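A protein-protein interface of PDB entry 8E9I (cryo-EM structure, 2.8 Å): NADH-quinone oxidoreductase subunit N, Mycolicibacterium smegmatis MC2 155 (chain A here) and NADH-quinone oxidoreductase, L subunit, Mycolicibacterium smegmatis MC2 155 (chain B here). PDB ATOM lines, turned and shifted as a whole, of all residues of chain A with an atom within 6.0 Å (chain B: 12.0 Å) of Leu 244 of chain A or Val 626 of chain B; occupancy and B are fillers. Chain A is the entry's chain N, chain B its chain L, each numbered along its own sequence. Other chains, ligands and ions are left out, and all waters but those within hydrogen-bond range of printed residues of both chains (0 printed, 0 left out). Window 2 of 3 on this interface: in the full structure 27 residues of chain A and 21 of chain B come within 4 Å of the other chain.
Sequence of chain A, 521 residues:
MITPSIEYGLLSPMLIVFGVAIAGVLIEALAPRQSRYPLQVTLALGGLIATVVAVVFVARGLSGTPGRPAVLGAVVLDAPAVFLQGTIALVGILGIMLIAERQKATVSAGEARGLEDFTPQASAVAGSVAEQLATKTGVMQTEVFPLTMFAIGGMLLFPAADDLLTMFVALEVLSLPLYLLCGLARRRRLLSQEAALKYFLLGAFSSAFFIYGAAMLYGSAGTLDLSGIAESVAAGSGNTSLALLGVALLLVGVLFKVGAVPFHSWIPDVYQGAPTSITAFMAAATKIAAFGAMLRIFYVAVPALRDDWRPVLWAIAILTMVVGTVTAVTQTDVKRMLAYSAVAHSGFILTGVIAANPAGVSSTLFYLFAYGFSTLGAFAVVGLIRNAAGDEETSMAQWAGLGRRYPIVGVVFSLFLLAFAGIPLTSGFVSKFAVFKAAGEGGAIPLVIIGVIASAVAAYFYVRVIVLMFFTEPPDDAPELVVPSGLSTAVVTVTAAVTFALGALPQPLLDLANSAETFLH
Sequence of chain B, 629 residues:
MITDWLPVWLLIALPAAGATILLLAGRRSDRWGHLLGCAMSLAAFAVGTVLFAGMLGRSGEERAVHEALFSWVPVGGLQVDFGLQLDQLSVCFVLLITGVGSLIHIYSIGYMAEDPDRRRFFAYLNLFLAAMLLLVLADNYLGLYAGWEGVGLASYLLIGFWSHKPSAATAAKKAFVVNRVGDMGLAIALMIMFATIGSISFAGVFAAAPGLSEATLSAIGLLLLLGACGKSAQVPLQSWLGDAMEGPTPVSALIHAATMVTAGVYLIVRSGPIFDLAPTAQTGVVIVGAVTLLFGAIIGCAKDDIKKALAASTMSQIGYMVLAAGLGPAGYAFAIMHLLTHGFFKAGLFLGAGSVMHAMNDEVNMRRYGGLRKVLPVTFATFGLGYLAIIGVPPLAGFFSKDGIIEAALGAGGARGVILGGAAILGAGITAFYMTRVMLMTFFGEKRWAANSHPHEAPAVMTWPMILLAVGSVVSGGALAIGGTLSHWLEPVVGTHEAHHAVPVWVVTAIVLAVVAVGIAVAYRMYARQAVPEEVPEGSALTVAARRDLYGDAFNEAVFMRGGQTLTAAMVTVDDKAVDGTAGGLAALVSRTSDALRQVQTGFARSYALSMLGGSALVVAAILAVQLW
Leu 244 of chain A touches two residues of chain B.
Val 626 of chain B touches just one residue of chain A: Leu 244 (3.5 Å).
No residue of chain B comes within 4 Å of Thr 240 of chain A.
No residue of chain B comes within 4 Å of Ala 243 of chain A.
Leu 245 of chain A touches one residue of chain B.
Val 247 of chain A touches none of the printed residues of chain B.
Ala 248 of chain A touches one residue of chain B.
No residue of chain B comes within 4 Å of Leu 305 of chain A.
Printed residues of chain B within 4 Å of Asp 308 of chain A: Ala 625 (3.2 Å).
Of the printed residues of chain B, Leu 249 of chain A touches Val 619 (3.99 Å).
Of the printed residues of chain A, Ala 625 of chain B touches Asp 308 (3.2 Å).
Printed residues of chain A within 4 Å of Ala 622 of chain B: Leu 244 (3.9 Å).
Printed residues of chain A within 4 Å of Val 619 of chain B: Leu 245, Ala 248 and Leu 249.
Val 620 of chain B touches none of the printed residues of chain A.
Leu 217 of chain A touches none of the printed residues of chain B.
The nearest residue of chain B that does not touch Leu 244 of chain A is Ile 623 of chain B (4.6 Å).
The nearest residue of chain A that does not touch Val 626 of chain B is Thr 240 of chain A (5.4 Å).
The nearest printed residue of chain A that does not touch Val 619 of chain B is Leu 244 of chain A (6.2 Å).
Of the 15 printed residues of chain A, 5 touch a printed residue of chain B.
Printed residues of chain A that touch a printed residue of chain B: Leu 244, Leu 245, Ala 248, Leu 249 and Asp 308.
Among the printed residues, 6 pairs touch across the chains.
Among the printed residues, no Asp or Glu carboxylate lies within 4 Å of a Lys or Arg side-chain nitrogen of the other chain.
Leu 244 of chain A touches Ala 622 of chain B.
CD1 of Leu 244 of chain A touches CG1 of Val 626 of chain B, 3.5 Å away.
Leu 245 of chain A touches Val 619 of chain B.
Val 619 of chain B touches Ala 248 of chain A (CA to CB, 3.9 Å).
CD2 of Leu 249 of chain A touches CG2 of Val 619 of chain B, 3.99 Å away.
Ala 625 of chain B touches Asp 308 of chain A.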
ATOM      1  N   LEU A 217     -20.955  -6.520  10.881  1.00  0.00           N
ATOM      2  CA  LEU A 217     -22.076  -6.817  11.769  1.00  0.00           C
ATOM      3  C   LEU A 217     -22.000  -5.980  13.035  1.00  0.00           C
ATOM      4  O   LEU A 217     -23.011  -5.451  13.508  1.00  0.00           O
ATOM      5  CB  LEU A 217     -22.107  -8.305  12.119  1.00  0.00           C
ATOM      6  CG  LEU A 217     -22.774  -9.243  11.117  1.00  0.00           C
ATOM      7  CD1 LEU A 217     -22.646 -10.673  11.587  1.00  0.00           C
ATOM      8  CD2 LEU A 217     -24.234  -8.882  10.944  1.00  0.00           C
ATOM      9  N   ASN A 239     -27.938  -0.404  10.979  1.00  0.00           N
ATOM     10  CA  ASN A 239     -27.814  -0.203   9.543  1.00  0.00           C
ATOM     11  C   ASN A 239     -28.103  -1.511   8.820  1.00  0.00           C
ATOM     12  O   ASN A 239     -27.330  -2.468   8.924  1.00  0.00           O
ATOM     13  CB  ASN A 239     -26.414   0.298   9.210  1.00  0.00           C
ATOM     14  CG  ASN A 239     -26.230   0.578   7.736  1.00  0.00           C
ATOM     15  OD1 ASN A 239     -26.218  -0.337   6.916  1.00  0.00           O
ATOM     16  ND2 ASN A 239     -26.070   1.849   7.391  1.00  0.00           N
ATOM     17  N   THR A 240     -29.218  -1.556   8.089  1.00  0.00           N
ATOM     18  CA  THR A 240     -29.612  -2.794   7.425  1.00  0.00           C
ATOM     19  C   THR A 240     -28.583  -3.211   6.384  1.00  0.00           C
ATOM     20  O   THR A 240     -28.247  -4.396   6.270  1.00  0.00           O
ATOM     21  CB  THR A 240     -30.984  -2.628   6.775  1.00  0.00           C
ATOM     22  OG1 THR A 240     -31.907  -2.089   7.730  1.00  0.00           O
ATOM     23  CG2 THR A 240     -31.501  -3.964   6.273  1.00  0.00           C
ATOM     24  N   SER A 241     -28.076  -2.254   5.609  1.00  0.00           N
ATOM     25  CA  SER A 241     -27.093  -2.585   4.584  1.00  0.00           C
ATOM     26  C   SER A 241     -25.837  -3.183   5.203  1.00  0.00           C
ATOM     27  O   SER A 241     -25.300  -4.173   4.696  1.00  0.00           O
ATOM     28  CB  SER A 241     -26.747  -1.339   3.771  1.00  0.00           C
ATOM     29  OG  SER A 241     -26.064  -0.387   4.566  1.00  0.00           O
ATOM     30  N   LEU A 242     -25.354  -2.595   6.297  1.00  0.00           N
ATOM     31  CA  LEU A 242     -24.187  -3.155   6.966  1.00  0.00           C
ATOM     32  C   LEU A 242     -24.496  -4.525   7.543  1.00  0.00           C
ATOM     33  O   LEU A 242     -23.653  -5.424   7.505  1.00  0.00           O
ATOM     34  CB  LEU A 242     -23.702  -2.213   8.065  1.00  0.00           C
ATOM     35  CG  LEU A 242     -22.737  -1.099   7.657  1.00  0.00           C
ATOM     36  CD1 LEU A 242     -22.233  -0.384   8.889  1.00  0.00           C
ATOM     37  CD2 LEU A 242     -21.567  -1.642   6.868  1.00  0.00           C
ATOM     38  N   ALA A 243     -25.692  -4.706   8.097  1.00  0.00           N
ATOM     39  CA  ALA A 243     -26.059  -6.020   8.605  1.00  0.00           C
ATOM     40  C   ALA A 243     -25.978  -7.058   7.497  1.00  0.00           C
ATOM     41  O   ALA A 243     -25.415  -8.141   7.681  1.00  0.00           O
ATOM     42  CB  ALA A 243     -27.462  -5.978   9.204  1.00  0.00           C
ATOM     43  N   LEU A 244     -26.512  -6.725   6.323  1.00  0.00           N
ATOM     44  CA  LEU A 244     -26.487  -7.660   5.207  1.00  0.00           C
ATOM     45  C   LEU A 244     -25.065  -7.933   4.742  1.00  0.00           C
ATOM     46  O   LEU A 244     -24.697  -9.086   4.499  1.00  0.00           O
ATOM     47  CB  LEU A 244     -27.320  -7.111   4.056  1.00  0.00           C
ATOM     48  CG  LEU A 244     -28.814  -6.997   4.331  1.00  0.00           C
ATOM     49  CD1 LEU A 244     -29.484  -6.191   3.235  1.00  0.00           C
ATOM     50  CD2 LEU A 244     -29.439  -8.371   4.453  1.00  0.00           C
ATOM     51  N   LEU A 245     -24.255  -6.887   4.588  1.00  0.00           N
ATOM     52  CA  LEU A 245     -22.893  -7.085   4.110  1.00  0.00           C
ATOM     53  C   LEU A 245     -22.090  -7.919   5.097  1.00  0.00           C
ATOM     54  O   LEU A 245     -21.313  -8.795   4.697  1.00  0.00           O
ATOM     55  CB  LEU A 245     -22.222  -5.737   3.867  1.00  0.00           C
ATOM     56  CG  LEU A 245     -20.745  -5.790   3.484  1.00  0.00           C
ATOM     57  CD1 LEU A 245     -20.556  -6.544   2.179  1.00  0.00           C
ATOM     58  CD2 LEU A 245     -20.180  -4.391   3.366  1.00  0.00           C
ATOM     59  N   GLY A 246     -22.260  -7.658   6.391  1.00  0.00           N
ATOM     60  CA  GLY A 246     -21.574  -8.456   7.388  1.00  0.00           C
ATOM     61  C   GLY A 246     -22.033  -9.896   7.376  1.00  0.00           C
ATOM     62  O   GLY A 246     -21.229 -10.819   7.499  1.00  0.00           O
ATOM     63  N   VAL A 247     -23.339 -10.111   7.219  1.00  0.00           N
ATOM     64  CA  VAL A 247     -23.846 -11.474   7.133  1.00  0.00           C
ATOM     65  C   VAL A 247     -23.210 -12.184   5.950  1.00  0.00           C
ATOM     66  O   VAL A 247     -22.779 -13.334   6.052  1.00  0.00           O
ATOM     67  CB  VAL A 247     -25.381 -11.476   7.028  1.00  0.00           C
ATOM     68  CG1 VAL A 247     -25.878 -12.834   6.566  1.00  0.00           C
ATOM     69  CG2 VAL A 247     -25.997 -11.119   8.357  1.00  0.00           C
ATOM     70  N   ALA A 248     -23.137 -11.503   4.809  1.00  0.00           N
ATOM     71  CA  ALA A 248     -22.568 -12.121   3.618  1.00  0.00           C
ATOM     72  C   ALA A 248     -21.099 -12.459   3.826  1.00  0.00           C
ATOM     73  O   ALA A 248     -20.654 -13.569   3.512  1.00  0.00           O
ATOM     74  CB  ALA A 248     -22.742 -11.195   2.415  1.00  0.00           C
ATOM     75  N   LEU A 249     -20.328 -11.518   4.362  1.00  0.00           N
ATOM     76  CA  LEU A 249     -18.900 -11.767   4.537  1.00  0.00           C
ATOM     77  C   LEU A 249     -18.652 -12.871   5.556  1.00  0.00           C
ATOM     78  O   LEU A 249     -17.751 -13.697   5.378  1.00  0.00           O
ATOM     79  CB  LEU A 249     -18.194 -10.479   4.943  1.00  0.00           C
ATOM     80  CG  LEU A 249     -18.144  -9.411   3.850  1.00  0.00           C
ATOM     81  CD1 LEU A 249     -17.762  -8.064   4.438  1.00  0.00           C
ATOM     82  CD2 LEU A 249     -17.191  -9.810   2.744  1.00  0.00           C
ATOM     83  N   LEU A 305     -33.616 -11.302   9.135  1.00  0.00           N
ATOM     84  CA  LEU A 305     -33.202 -11.034   7.768  1.00  0.00           C
ATOM     85  C   LEU A 305     -33.314 -12.260   6.879  1.00  0.00           C
ATOM     86  O   LEU A 305     -32.597 -12.356   5.882  1.00  0.00           O
ATOM     87  CB  LEU A 305     -31.768 -10.511   7.743  1.00  0.00           C
ATOM     88  CG  LEU A 305     -31.455  -9.413   8.757  1.00  0.00           C
ATOM     89  CD1 LEU A 305     -30.040  -8.909   8.567  1.00  0.00           C
ATOM     90  CD2 LEU A 305     -32.449  -8.276   8.623  1.00  0.00           C
ATOM     91  N   ASP A 308     -33.814 -11.899   3.316  1.00  0.00           N
ATOM     92  CA  ASP A 308     -32.641 -11.309   2.693  1.00  0.00           C
ATOM     93  C   ASP A 308     -31.539 -12.320   2.414  1.00  0.00           C
ATOM     94  O   ASP A 308     -30.873 -12.215   1.383  1.00  0.00           O
ATOM     95  CB  ASP A 308     -32.088 -10.187   3.575  1.00  0.00           C
ATOM     96  N   TRP A 309     -31.321 -13.300   3.295  1.00  0.00           N
ATOM     97  CA  TRP A 309     -30.226 -14.240   3.077  1.00  0.00           C
ATOM     98  C   TRP A 309     -30.703 -15.604   2.615  1.00  0.00           C
ATOM     99  O   TRP A 309     -29.879 -16.438   2.227  1.00  0.00           O
ATOM    100  CB  TRP A 309     -29.377 -14.411   4.345  1.00  0.00           C
ATOM    101  CG  TRP A 309     -30.114 -14.813   5.584  1.00  0.00           C
ATOM    102  CD1 TRP A 309     -30.462 -14.004   6.619  1.00  0.00           C
ATOM    103  CD2 TRP A 309     -30.554 -16.129   5.938  1.00  0.00           C
ATOM    104  NE1 TRP A 309     -31.108 -14.727   7.588  1.00  0.00           N
ATOM    105  CE2 TRP A 309     -31.175 -16.036   7.194  1.00  0.00           C
ATOM    106  CE3 TRP A 309     -30.488 -17.374   5.313  1.00  0.00           C
ATOM    107  CZ2 TRP A 309     -31.731 -17.136   7.834  1.00  0.00           C
ATOM    108  CZ3 TRP A 309     -31.042 -18.467   5.953  1.00  0.00           C
ATOM    109  CH2 TRP A 309     -31.653 -18.340   7.199  1.00  0.00           C
ATOM    110  N   GLY B 615     -16.625 -15.209  -4.895  1.00  0.00           N
ATOM    111  CA  GLY B 615     -17.685 -15.405  -3.923  1.00  0.00           C
ATOM    112  C   GLY B 615     -18.349 -14.122  -3.469  1.00  0.00           C
ATOM    113  O   GLY B 615     -19.405 -14.185  -2.833  1.00  0.00           O
ATOM    114  N   SER B 616     -17.763 -12.960  -3.783  1.00  0.00           N
ATOM    115  CA  SER B 616     -18.478 -11.696  -3.649  1.00  0.00           C
ATOM    116  C   SER B 616     -19.779 -11.705  -4.432  1.00  0.00           C
ATOM    117  O   SER B 616     -20.569 -10.761  -4.326  1.00  0.00           O
ATOM    118  CB  SER B 616     -17.610 -10.540  -4.133  1.00  0.00           C
ATOM    119  OG  SER B 616     -17.291 -10.697  -5.502  1.00  0.00           O
ATOM    120  N   ALA B 617     -20.001 -12.737  -5.245  1.00  0.00           N
ATOM    121  CA  ALA B 617     -21.346 -13.017  -5.718  1.00  0.00           C
ATOM    122  C   ALA B 617     -22.314 -13.063  -4.545  1.00  0.00           C
ATOM    123  O   ALA B 617     -23.438 -12.561  -4.635  1.00  0.00           O
ATOM    124  CB  ALA B 617     -21.365 -14.337  -6.489  1.00  0.00           C
ATOM    125  N   LEU B 618     -21.883 -13.648  -3.425  1.00  0.00           N
ATOM    126  CA  LEU B 618     -22.712 -13.647  -2.227  1.00  0.00           C
ATOM    127  C   LEU B 618     -22.990 -12.231  -1.749  1.00  0.00           C
ATOM    128  O   LEU B 618     -24.125 -11.906  -1.386  1.00  0.00           O
ATOM    129  CB  LEU B 618     -22.036 -14.445  -1.117  1.00  0.00           C
ATOM    130  CG  LEU B 618     -22.215 -15.956  -1.186  1.00  0.00           C
ATOM    131  CD1 LEU B 618     -21.639 -16.516  -2.468  1.00  0.00           C
ATOM    132  CD2 LEU B 618     -21.567 -16.611   0.016  1.00  0.00           C
ATOM    133  N   VAL B 619     -21.966 -11.379  -1.722  1.00  0.00           N
ATOM    134  CA  VAL B 619     -22.159 -10.016  -1.242  1.00  0.00           C
ATOM    135  C   VAL B 619     -23.166  -9.293  -2.120  1.00  0.00           C
ATOM    136  O   VAL B 619     -24.099  -8.648  -1.630  1.00  0.00           O
ATOM    137  CB  VAL B 619     -20.820  -9.264  -1.201  1.00  0.00           C
ATOM    138  CG1 VAL B 619     -21.049  -7.804  -0.851  1.00  0.00           C
ATOM    139  CG2 VAL B 619     -19.885  -9.908  -0.202  1.00  0.00           C
ATOM    140  N   VAL B 620     -22.993  -9.397  -3.434  1.00  0.00           N
ATOM    141  CA  VAL B 620     -23.871  -8.672  -4.342  1.00  0.00           C
ATOM    142  C   VAL B 620     -25.284  -9.226  -4.264  1.00  0.00           C
ATOM    143  O   VAL B 620     -26.261  -8.474  -4.331  1.00  0.00           O
ATOM    144  CB  VAL B 620     -23.324  -8.713  -5.779  1.00  0.00           C
ATOM    145  CG1 VAL B 620     -23.221 -10.136  -6.273  1.00  0.00           C
ATOM    146  CG2 VAL B 620     -24.214  -7.897  -6.698  1.00  0.00           C
ATOM    147  N   ALA B 621     -25.422 -10.544  -4.109  1.00  0.00           N
ATOM    148  CA  ALA B 621     -26.748 -11.139  -4.018  1.00  0.00           C
ATOM    149  C   ALA B 621     -27.458 -10.708  -2.741  1.00  0.00           C
ATOM    150  O   ALA B 621     -28.642 -10.363  -2.765  1.00  0.00           O
ATOM    151  CB  ALA B 621     -26.641 -12.661  -4.091  1.00  0.00           C
ATOM    152  N   ALA B 622     -26.753 -10.725  -1.610  1.00  0.00           N
ATOM    153  CA  ALA B 622     -27.376 -10.295  -0.364  1.00  0.00           C
ATOM    154  C   ALA B 622     -27.720  -8.814  -0.400  1.00  0.00           C
ATOM    155  O   ALA B 622     -28.755  -8.404   0.137  1.00  0.00           O
ATOM    156  CB  ALA B 622     -26.459 -10.598   0.819  1.00  0.00           C
ATOM    157  N   ILE B 623     -26.869  -7.995  -1.020  1.00  0.00           N
ATOM    158  CA  ILE B 623     -27.155  -6.570  -1.117  1.00  0.00           C
ATOM    159  C   ILE B 623     -28.350  -6.333  -2.031  1.00  0.00           C
ATOM    160  O   ILE B 623     -29.178  -5.451  -1.780  1.00  0.00           O
ATOM    161  CB  ILE B 623     -25.910  -5.809  -1.606  1.00  0.00           C
ATOM    162  CG1 ILE B 623     -24.811  -5.828  -0.540  1.00  0.00           C
ATOM    163  CG2 ILE B 623     -26.267  -4.377  -1.965  1.00  0.00           C
ATOM    164  CD1 ILE B 623     -25.109  -4.993   0.684  1.00  0.00           C
ATOM    165  N   LEU B 624     -28.452  -7.111  -3.108  1.00  0.00           N
ATOM    166  CA  LEU B 624     -29.555  -6.950  -4.045  1.00  0.00           C
ATOM    167  C   LEU B 624     -30.832  -7.597  -3.537  1.00  0.00           C
ATOM    168  O   LEU B 624     -31.907  -7.345  -4.091  1.00  0.00           O
ATOM    169  CB  LEU B 624     -29.170  -7.543  -5.398  1.00  0.00           C
ATOM    170  N   ALA B 625     -30.738  -8.432  -2.501  1.00  0.00           N
ATOM    171  CA  ALA B 625     -31.931  -9.047  -1.940  1.00  0.00           C
ATOM    172  C   ALA B 625     -32.900  -8.008  -1.406  1.00  0.00           C
ATOM    173  O   ALA B 625     -34.075  -8.325  -1.193  1.00  0.00           O
ATOM    174  CB  ALA B 625     -31.550 -10.023  -0.828  1.00  0.00           C
ATOM    175  N   VAL B 626     -32.433  -6.779  -1.173  1.00  0.00           N
ATOM    176  CA  VAL B 626     -33.329  -5.697  -0.790  1.00  0.00           C
ATOM    177  C   VAL B 626     -34.222  -5.260  -1.937  1.00  0.00           C
ATOM    178  O   VAL B 626     -35.190  -4.526  -1.713  1.00  0.00           O
ATOM    179  CB  VAL B 626     -32.542  -4.469  -0.293  1.00  0.00           C
ATOM    180  CG1 VAL B 626     -31.701  -4.825   0.925  1.00  0.00           C
ATOM    181  CG2 VAL B 626     -31.695  -3.884  -1.417  1.00  0.00           C
ATOM    182  N   GLN B 627     -33.920  -5.690  -3.157  1.00  0.00           N
ATOM    183  CA  GLN B 627     -34.638  -5.229  -4.336  1.00  0.00           C
ATOM    184  C   GLN B 627     -34.801  -6.355  -5.350  1.00  0.00           C
ATOM    185  O   GLN B 627     -34.543  -6.176  -6.539  1.00  0.00           O
ATOM    186  CB  GLN B 627     -33.900  -4.048  -4.966  1.00  0.00           C
ATOM    187  CG  GLN B 627     -32.459  -4.353  -5.337  1.00  0.00           C
ATOM    188  CD  GLN B 627     -31.745  -3.157  -5.928  1.00  0.00           C
ATOM    189  OE1 GLN B 627     -32.191  -2.580  -6.918  1.00  0.00           O
ATOM    190  NE2 GLN B 627     -30.617  -2.788  -5.332  1.00  0.00           N
